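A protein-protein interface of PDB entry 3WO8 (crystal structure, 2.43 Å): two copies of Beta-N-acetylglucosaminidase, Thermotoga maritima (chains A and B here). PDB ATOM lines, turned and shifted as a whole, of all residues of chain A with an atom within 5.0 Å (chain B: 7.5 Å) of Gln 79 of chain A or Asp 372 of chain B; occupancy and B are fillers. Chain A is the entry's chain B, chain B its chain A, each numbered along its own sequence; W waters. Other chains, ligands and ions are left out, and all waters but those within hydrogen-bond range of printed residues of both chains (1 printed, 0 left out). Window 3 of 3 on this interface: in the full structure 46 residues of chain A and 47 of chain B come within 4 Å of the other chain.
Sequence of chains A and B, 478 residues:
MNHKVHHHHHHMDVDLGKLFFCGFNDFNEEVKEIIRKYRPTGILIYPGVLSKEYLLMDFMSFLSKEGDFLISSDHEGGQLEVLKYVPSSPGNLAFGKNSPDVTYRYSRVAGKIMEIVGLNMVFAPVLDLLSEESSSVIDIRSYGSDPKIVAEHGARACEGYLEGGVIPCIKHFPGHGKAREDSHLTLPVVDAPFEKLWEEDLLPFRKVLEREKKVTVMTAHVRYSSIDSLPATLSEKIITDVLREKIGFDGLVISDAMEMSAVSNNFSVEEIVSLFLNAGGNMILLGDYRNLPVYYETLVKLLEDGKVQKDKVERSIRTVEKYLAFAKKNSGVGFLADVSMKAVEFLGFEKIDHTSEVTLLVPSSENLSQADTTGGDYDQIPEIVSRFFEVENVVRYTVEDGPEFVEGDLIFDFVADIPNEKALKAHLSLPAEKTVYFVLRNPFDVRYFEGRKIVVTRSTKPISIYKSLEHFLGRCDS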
ATOM      1  N   GLY A  77      32.011  -1.433 -29.075  1.00  0.00           N
ATOM      2  CA  GLY A  77      30.715  -1.320 -29.764  1.00  0.00           C
ATOM      3  C   GLY A  77      29.929  -2.580 -29.453  1.00  0.00           C
ATOM      4  O   GLY A  77      30.510  -3.639 -29.231  1.00  0.00           O
ATOM      5  N   GLY A  78      28.622  -2.467 -29.365  1.00  0.00           N
ATOM      6  CA  GLY A  78      27.816  -3.606 -29.018  1.00  0.00           C
ATOM      7  C   GLY A  78      27.855  -3.769 -27.524  1.00  0.00           C
ATOM      8  O   GLY A  78      27.660  -2.779 -26.789  1.00  0.00           O
ATOM      9  N   GLN A  79      28.085  -5.014 -27.090  1.00  0.00           N
ATOM     10  CA  GLN A  79      28.141  -5.411 -25.690  1.00  0.00           C
ATOM     11  C   GLN A  79      28.984  -4.508 -24.793  1.00  0.00           C
ATOM     12  O   GLN A  79      28.573  -4.185 -23.673  1.00  0.00           O
ATOM     13  CB  GLN A  79      28.718  -6.806 -25.559  1.00  0.00           C
ATOM     14  CG  GLN A  79      28.364  -7.448 -24.232  1.00  0.00           C
ATOM     15  CD  GLN A  79      29.079  -8.765 -23.988  1.00  0.00           C
ATOM     16  OE1 GLN A  79      28.896  -9.746 -24.722  1.00  0.00           O
ATOM     17  NE2 GLN A  79      29.874  -8.799 -22.934  1.00  0.00           N
ATOM     18  N   LEU A  80      30.155  -4.101 -25.276  1.00  0.00           N
ATOM     19  CA  LEU A  80      31.034  -3.306 -24.474  1.00  0.00           C
ATOM     20  C   LEU A  80      31.055  -1.932 -25.043  1.00  0.00           C
ATOM     21  O   LEU A  80      31.614  -1.720 -26.120  1.00  0.00           O
ATOM     22  CB  LEU A  80      32.450  -3.900 -24.436  1.00  0.00           C
ATOM     23  CG  LEU A  80      32.786  -4.862 -23.314  1.00  0.00           C
ATOM     24  CD1 LEU A  80      31.602  -5.764 -23.033  1.00  0.00           C
ATOM     25  CD2 LEU A  80      34.019  -5.682 -23.683  1.00  0.00           C
ATOM     26  N   GLU A  81      30.444  -1.000 -24.323  1.00  0.00           N
ATOM     27  CA  GLU A  81      30.368   0.394 -24.780  1.00  0.00           C
ATOM     28  C   GLU A  81      30.540   1.288 -23.580  1.00  0.00           C
ATOM     29  O   GLU A  81      29.931   1.064 -22.586  1.00  0.00           O
ATOM     30  CB  GLU A  81      29.042   0.695 -25.499  1.00  0.00           C
ATOM     31  CG  GLU A  81      28.899  -0.016 -26.826  1.00  0.00           C
ATOM     32  CD  GLU A  81      27.654   0.382 -27.651  1.00  0.00           C
ATOM     33  OE1 GLU A  81      26.621   0.777 -27.061  1.00  0.00           O
ATOM     34  OE2 GLU A  81      27.724   0.299 -28.906  1.00  0.00           O
ATOM     35  N   ASP A 139      30.720 -14.522 -27.695  1.00  0.00           N
ATOM     36  CA  ASP A 139      29.694 -14.711 -28.730  1.00  0.00           C
ATOM     37  C   ASP A 139      29.301 -13.427 -29.506  1.00  0.00           C
ATOM     38  O   ASP A 139      29.677 -13.285 -30.685  1.00  0.00           O
ATOM     39  CB  ASP A 139      28.444 -15.494 -28.214  1.00  0.00           C
ATOM     40  CG  ASP A 139      27.838 -14.928 -26.922  1.00  0.00           C
ATOM     41  OD1 ASP A 139      27.690 -13.685 -26.825  1.00  0.00           O
ATOM     42  OD2 ASP A 139      27.473 -15.739 -26.025  1.00  0.00           O
ATOM     43  N   ILE A 140      28.579 -12.493 -28.868  1.00  0.00           N
ATOM     44  CA  ILE A 140      28.166 -11.263 -29.572  1.00  0.00           C
ATOM     45  C   ILE A 140      29.292 -10.288 -29.839  1.00  0.00           C
ATOM     46  O   ILE A 140      29.149  -9.436 -30.702  1.00  0.00           O
ATOM     47  CB  ILE A 140      27.000 -10.492 -28.918  1.00  0.00           C
ATOM     48  CG1 ILE A 140      27.331 -10.026 -27.491  1.00  0.00           C
ATOM     49  CG2 ILE A 140      25.748 -11.349 -28.927  1.00  0.00           C
ATOM     50  CD1 ILE A 140      26.438  -8.900 -27.000  1.00  0.00           C
ATOM     51  N   ARG A 141      30.404 -10.457 -29.140  1.00  0.00           N
ATOM     52  CA  ARG A 141      31.611  -9.661 -29.348  1.00  0.00           C
ATOM     53  C   ARG A 141      32.538 -10.105 -30.481  1.00  0.00           C
ATOM     54  O   ARG A 141      33.604  -9.492 -30.691  1.00  0.00           O
ATOM     55  CB  ARG A 141      32.454  -9.710 -28.080  1.00  0.00           C
ATOM     56  CG  ARG A 141      31.907  -8.908 -26.940  1.00  0.00           C
ATOM     57  CD  ARG A 141      32.743  -9.120 -25.703  1.00  0.00           C
ATOM     58  NE  ARG A 141      34.109  -8.635 -25.897  1.00  0.00           N
ATOM     59  CZ  ARG A 141      35.128  -8.939 -25.106  1.00  0.00           C
ATOM     60  NH1 ARG A 141      34.954  -9.746 -24.077  1.00  0.00           N
ATOM     61  NH2 ARG A 141      36.332  -8.447 -25.351  1.00  0.00           N
ATOM     62  N   GLU B 366      22.661 -10.394 -15.068  1.00  0.00           N
ATOM     63  CA  GLU B 366      23.684 -11.197 -14.378  1.00  0.00           C
ATOM     64  C   GLU B 366      25.065 -10.527 -14.321  1.00  0.00           C
ATOM     65  O   GLU B 366      25.842 -10.774 -13.382  1.00  0.00           O
ATOM     66  CB  GLU B 366      23.826 -12.581 -15.038  1.00  0.00           C
ATOM     67  CG  GLU B 366      24.779 -13.544 -14.322  1.00  0.00           C
ATOM     68  CD  GLU B 366      24.411 -13.800 -12.865  1.00  0.00           C
ATOM     69  OE1 GLU B 366      25.328 -13.792 -12.013  1.00  0.00           O
ATOM     70  OE2 GLU B 366      23.213 -14.005 -12.568  1.00  0.00           O
ATOM     71  N   ASN B 367      25.377  -9.704 -15.326  1.00  0.00           N
ATOM     72  CA  ASN B 367      26.687  -9.081 -15.405  1.00  0.00           C
ATOM     73  C   ASN B 367      26.690  -7.649 -14.939  1.00  0.00           C
ATOM     74  O   ASN B 367      25.882  -6.858 -15.374  1.00  0.00           O
ATOM     75  CB  ASN B 367      27.222  -9.136 -16.813  1.00  0.00           C
ATOM     76  CG  ASN B 367      28.696  -8.784 -16.875  1.00  0.00           C
ATOM     77  OD1 ASN B 367      29.104  -7.678 -16.537  1.00  0.00           O
ATOM     78  ND2 ASN B 367      29.501  -9.723 -17.298  1.00  0.00           N
ATOM     79  N   LEU B 368      27.622  -7.317 -14.057  1.00  0.00           N
ATOM     80  CA  LEU B 368      27.696  -5.973 -13.499  1.00  0.00           C
ATOM     81  C   LEU B 368      29.010  -5.285 -13.775  1.00  0.00           C
ATOM     82  O   LEU B 368      29.339  -4.318 -13.116  1.00  0.00           O
ATOM     83  CB  LEU B 368      27.510  -6.042 -11.991  1.00  0.00           C
ATOM     84  CG  LEU B 368      26.157  -5.679 -11.405  1.00  0.00           C
ATOM     85  CD1 LEU B 368      25.036  -6.456 -12.050  1.00  0.00           C
ATOM     86  CD2 LEU B 368      26.251  -6.005  -9.938  1.00  0.00           C
ATOM     87  N   SER B 369      29.783  -5.786 -14.724  1.00  0.00           N
ATOM     88  CA  SER B 369      31.018  -5.125 -15.080  1.00  0.00           C
ATOM     89  C   SER B 369      30.672  -3.802 -15.746  1.00  0.00           C
ATOM     90  O   SER B 369      29.682  -3.700 -16.496  1.00  0.00           O
ATOM     91  CB  SER B 369      31.849  -5.972 -16.035  1.00  0.00           C
ATOM     92  OG  SER B 369      32.676  -5.126 -16.837  1.00  0.00           O
ATOM     93  N   GLN B 370      31.515  -2.812 -15.484  1.00  0.00           N
ATOM     94  CA  GLN B 370      31.268  -1.422 -15.882  1.00  0.00           C
ATOM     95  C   GLN B 370      31.051  -1.147 -17.367  1.00  0.00           C
ATOM     96  O   GLN B 370      30.333  -0.224 -17.706  1.00  0.00           O
ATOM     97  CB  GLN B 370      32.456  -0.560 -15.507  1.00  0.00           C
ATOM     98  CG  GLN B 370      32.743  -0.384 -14.048  1.00  0.00           C
ATOM     99  CD  GLN B 370      33.953   0.507 -13.872  1.00  0.00           C
ATOM    100  OE1 GLN B 370      35.102   0.138 -14.236  1.00  0.00           O
ATOM    101  NE2 GLN B 370      33.703   1.710 -13.332  1.00  0.00           N
ATOM    102  N   ALA B 371      31.748  -1.868 -18.232  1.00  0.00           N
ATOM    103  CA  ALA B 371      31.643  -1.664 -19.681  1.00  0.00           C
ATOM    104  C   ALA B 371      30.586  -2.530 -20.345  1.00  0.00           C
ATOM    105  O   ALA B 371      30.222  -2.276 -21.499  1.00  0.00           O
ATOM    106  CB  ALA B 371      32.983  -1.912 -20.348  1.00  0.00           C
ATOM    107  N   ASP B 372      30.124  -3.563 -19.654  1.00  0.00           N
ATOM    108  CA  ASP B 372      29.094  -4.402 -20.206  1.00  0.00           C
ATOM    109  C   ASP B 372      27.737  -3.689 -20.103  1.00  0.00           C
ATOM    110  O   ASP B 372      27.366  -3.251 -19.039  1.00  0.00           O
ATOM    111  CB  ASP B 372      29.050  -5.725 -19.483  1.00  0.00           C
ATOM    112  CG  ASP B 372      28.113  -6.706 -20.140  1.00  0.00           C
ATOM    113  OD1 ASP B 372      27.083  -6.265 -20.650  1.00  0.00           O
ATOM    114  OD2 ASP B 372      28.386  -7.926 -20.149  1.00  0.00           O
ATOM    115  N   THR B 373      27.034  -3.597 -21.233  1.00  0.00           N
ATOM    116  CA  THR B 373      25.741  -2.908 -21.377  1.00  0.00           C
ATOM    117  C   THR B 373      24.486  -3.805 -21.496  1.00  0.00           C
ATOM    118  O   THR B 373      23.359  -3.327 -21.611  1.00  0.00           O
ATOM    119  CB  THR B 373      25.769  -2.103 -22.663  1.00  0.00           C
ATOM    120  OG1 THR B 373      25.951  -2.977 -23.782  1.00  0.00           O
ATOM    121  CG2 THR B 373      26.872  -1.060 -22.620  1.00  0.00           C
ATOM    122  N   THR B 374      24.710  -5.103 -21.520  1.00  0.00           N
ATOM    123  CA  THR B 374      23.676  -6.143 -21.505  1.00  0.00           C
ATOM    124  C   THR B 374      22.515  -5.910 -20.515  1.00  0.00           C
ATOM    125  O   THR B 374      21.336  -5.970 -20.864  1.00  0.00           O
ATOM    126  CB  THR B 374      24.400  -7.487 -21.176  1.00  0.00           C
ATOM    127  OG1 THR B 374      25.174  -7.865 -22.311  1.00  0.00           O
ATOM    128  CG2 THR B 374      23.468  -8.573 -20.926  1.00  0.00           C
ATOM    129  N   GLY B 375      22.878  -5.689 -19.265  1.00  0.00           N
ATOM    130  CA  GLY B 375      21.924  -5.423 -18.200  1.00  0.00           C
ATOM    131  C   GLY B 375      20.891  -4.387 -18.552  1.00  0.00           C
ATOM    132  O   GLY B 375      19.685  -4.651 -18.490  1.00  0.00           O
ATOM    133  N   GLY B 376      21.371  -3.215 -18.926  1.00  0.00           N
ATOM    134  CA  GLY B 376      20.501  -2.081 -19.258  1.00  0.00           C
ATOM    135  C   GLY B 376      19.667  -2.416 -20.484  1.00  0.00           C
ATOM    136  O   GLY B 376      18.499  -2.085 -20.586  1.00  0.00           O
ATOM    137  N   ASP B 377      20.281  -3.112 -21.419  1.00  0.00           N
ATOM    138  CA  ASP B 377      19.577  -3.509 -22.592  1.00  0.00           C
ATOM    139  C   ASP B 377      18.367  -4.320 -22.182  1.00  0.00           C
ATOM    140  O   ASP B 377      17.297  -4.071 -22.691  1.00  0.00           O
ATOM    141  CB  ASP B 377      20.485  -4.303 -23.521  1.00  0.00           C
ATOM    142  CG  ASP B 377      21.498  -3.436 -24.275  1.00  0.00           C
ATOM    143  OD1 ASP B 377      21.449  -2.169 -24.229  1.00  0.00           O
ATOM    144  OD2 ASP B 377      22.354  -4.056 -24.954  1.00  0.00           O
ATOM    145  N   ARG B 441      21.668 -13.809 -28.077  1.00  0.00           N
ATOM    146  CA  ARG B 441      23.119 -13.887 -28.152  1.00  0.00           C
ATOM    147  C   ARG B 441      23.637 -14.862 -29.198  1.00  0.00           C
ATOM    148  O   ARG B 441      23.892 -14.478 -30.329  1.00  0.00           O
ATOM    149  CB  ARG B 441      23.714 -14.174 -26.794  1.00  0.00           C
ATOM    150  CG  ARG B 441      23.768 -12.944 -25.915  1.00  0.00           C
ATOM    151  CD  ARG B 441      23.984 -13.368 -24.497  1.00  0.00           C
ATOM    152  NE  ARG B 441      24.573 -12.322 -23.685  1.00  0.00           N
ATOM    153  CZ  ARG B 441      25.860 -12.021 -23.669  1.00  0.00           C
ATOM    154  NH1 ARG B 441      26.722 -12.667 -24.453  1.00  0.00           N
ATOM    155  NH2 ARG B 441      26.271 -11.044 -22.877  1.00  0.00           N
ATOM    156  N   SER B 459      22.287  -9.715 -31.303  1.00  0.00           N
ATOM    157  CA  SER B 459      22.619  -8.676 -30.340  1.00  0.00           C
ATOM    158  C   SER B 459      21.471  -8.475 -29.368  1.00  0.00           C
ATOM    159  O   SER B 459      20.314  -8.871 -29.612  1.00  0.00           O
ATOM    160  CB  SER B 459      23.059  -7.349 -31.023  1.00  0.00           C
ATOM    161  OG  SER B 459      22.218  -6.247 -30.796  1.00  0.00           O
ATOM    162  N   THR B 460      21.846  -7.894 -28.239  1.00  0.00           N
ATOM    163  CA  THR B 460      20.954  -7.582 -27.145  1.00  0.00           C
ATOM    164  C   THR B 460      20.555  -6.115 -27.183  1.00  0.00           C
ATOM    165  O   THR B 460      19.888  -5.626 -26.294  1.00  0.00           O
ATOM    166  CB  THR B 460      21.693  -7.791 -25.821  1.00  0.00           C
ATOM    167  OG1 THR B 460      22.661  -6.760 -25.631  1.00  0.00           O
ATOM    168  CG2 THR B 460      22.397  -9.106 -25.824  1.00  0.00           C
ATOM    169  N   LYS B 461      21.039  -5.396 -28.184  1.00  0.00           N
ATOM    170  CA  LYS B 461      20.787  -3.991 -28.287  1.00  0.00           C
ATOM    171  C   LYS B 461      19.325  -3.670 -28.638  1.00  0.00           C
ATOM    172  O   LYS B 461      18.694  -4.431 -29.345  1.00  0.00           O
ATOM    173  CB  LYS B 461      21.733  -3.414 -29.313  1.00  0.00           C
ATOM    174  CG  LYS B 461      23.185  -3.438 -28.844  1.00  0.00           C
ATOM    175  CD  LYS B 461      23.320  -2.591 -27.596  1.00  0.00           C
ATOM    176  CE  LYS B 461      24.648  -1.879 -27.490  1.00  0.00           C
ATOM    177  NZ  LYS B 461      25.192  -2.076 -26.123  1.00  0.00           N
HETATM  178  O   HOH W   1      31.196  -8.182 -20.202  1.00  0.00           O
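Water W1 lies within hydrogen-bond range of the side-chain carboxylate (OD2) of Asp 372 of chain B (2.8 Å) and the side-chain amide nitrogen (NE2) of Gln 79 of chain A (3.1 Å).
Of chain B, only Ala 371, Asp 372, Thr 373, Thr 374 and Arg 441 come within 4 Å of Gln 79 of chain A. Of the printed residues of chain B, Asp 139 of chain A touches Arg 441 (2.8 Å). Ser 369 of chain B touches none of the printed residues of chain A. Printed residues of chain A within 4 Å of Asp 372 of chain B: Gln 79. Of the printed residues of chain A, Thr 373 of chain B touches Gly 78 (3.5 Å), Gln 79 (2.9 Å) and Glu 81 (3.7 Å). Of the printed residues of chain A, Thr 374 of chain B touches Gln 79 (3.7 Å). Of the printed residues of chain A, Lys 461 of chain B touches Gly 78 (2.7 Å) and Glu 81 (3.3 Å). The nearest residue of chain B that does not touch Gln 79 of chain A is Lys 461 of chain B (4.2 Å).
The backbone NH (N) of Glu 81 of chain A sits at hydrogen-bond distance from the backbone carbonyl oxygen (O) of Ala 371 of chain B. The side-chain carboxylate (OD2) of Asp 372 of chain B lies within hydrogen-bond range of the side-chain amide nitrogen (NE2) of Gln 79 of chain A (3.3 Å). The backbone carbonyl oxygen of Gly 78 of chain A lies within hydrogen-bond range of the side-chain hydroxyl of Thr 373 of chain B (3.5 Å). OG1 of Thr 373 of chain B sits at hydrogen-bond distance from O of Gln 79 of chain A (2.9 Å). The guanidinium group of Arg 441 of chain B lies within hydrogen-bond range of the side-chain amide oxygen of Gln 79 of chain A (3.5 Å). The side-chain carboxylate (OD1) of Asp 139 of chain A lies within salt-bridge range of the guanidinium group (NH1) of Arg 441 of chain B, at 2.8 Å. The backbone carbonyl oxygen of Gly 78 of chain A lies within hydrogen-bond range of the side-chain amino group of Lys 461 of chain B, 2.7 Å away. The side-chain amino group (NZ) of Lys 461 of chain B is in salt-bridge range of the side-chain carboxylate (OE1) of Glu 81 of chain A, 3.3 Å away. O of Gln 79 of chain A lies close to O of Ala 371 of chain B (3.3 Å).
OD1 of Asp 372 of chain B lies within hydrogen-bond range of N of Thr 374 of chain B (2.8 Å). The side-chain hydroxyl of Thr 373 of chain B sits at hydrogen-bond distance from the side-chain amino group of Lys 461 of chain B, at 2.6 Å. OG1 of Thr 374 of chain B is in hydrogen-bond range of NH2 of Arg 441 of chain B, at 3.4 Å. OD2 of Asp 377 of chain B lies within salt-bridge range of NZ of Lys 461 of chain B, 3.7 Å away. The backbone NH of Lys 461 of chain B lies within hydrogen-bond range of the side-chain hydroxyl of Ser 459 of chain B. The backbone NH (N) of Gly 78 of chain A lies within hydrogen-bond range of the side-chain carboxylate (OE2) of Glu 81 of chain A.
Of the 8 printed residues of chain A, 6 touch a printed residue of chain B. Hydrophobic or aromatic side chains of chain A that line the printed part of chain B: Ile 140. Among the printed residues, 13 pairs touch across the chains. Among the printed residues, Asp or Glu carboxylates within 4 Å of a Lys or Arg side-chain nitrogen of the other chain: Glu 81 of chain A with Lys 461 of chain B (3.3 Å) and Asp 139 of chain A with Arg 441 of chain B (2.8 Å).
No position is printed for both chains. Of the 13 pairs that touch across the chains among the printed residues, none has its exchanged pair printed and touching as well.
Among the printed residues, merely in contact across the chains: Leu 80 of chain A with Ala 371 of chain B (3.3 Å), Glu 81 of chain A with Thr 373 of chain B (3.7 Å), Ile 140 of chain A with Arg 441 of chain B (3.7 Å) and Gln 79 of chain A with Thr 374 of chain B (3.7 Å).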
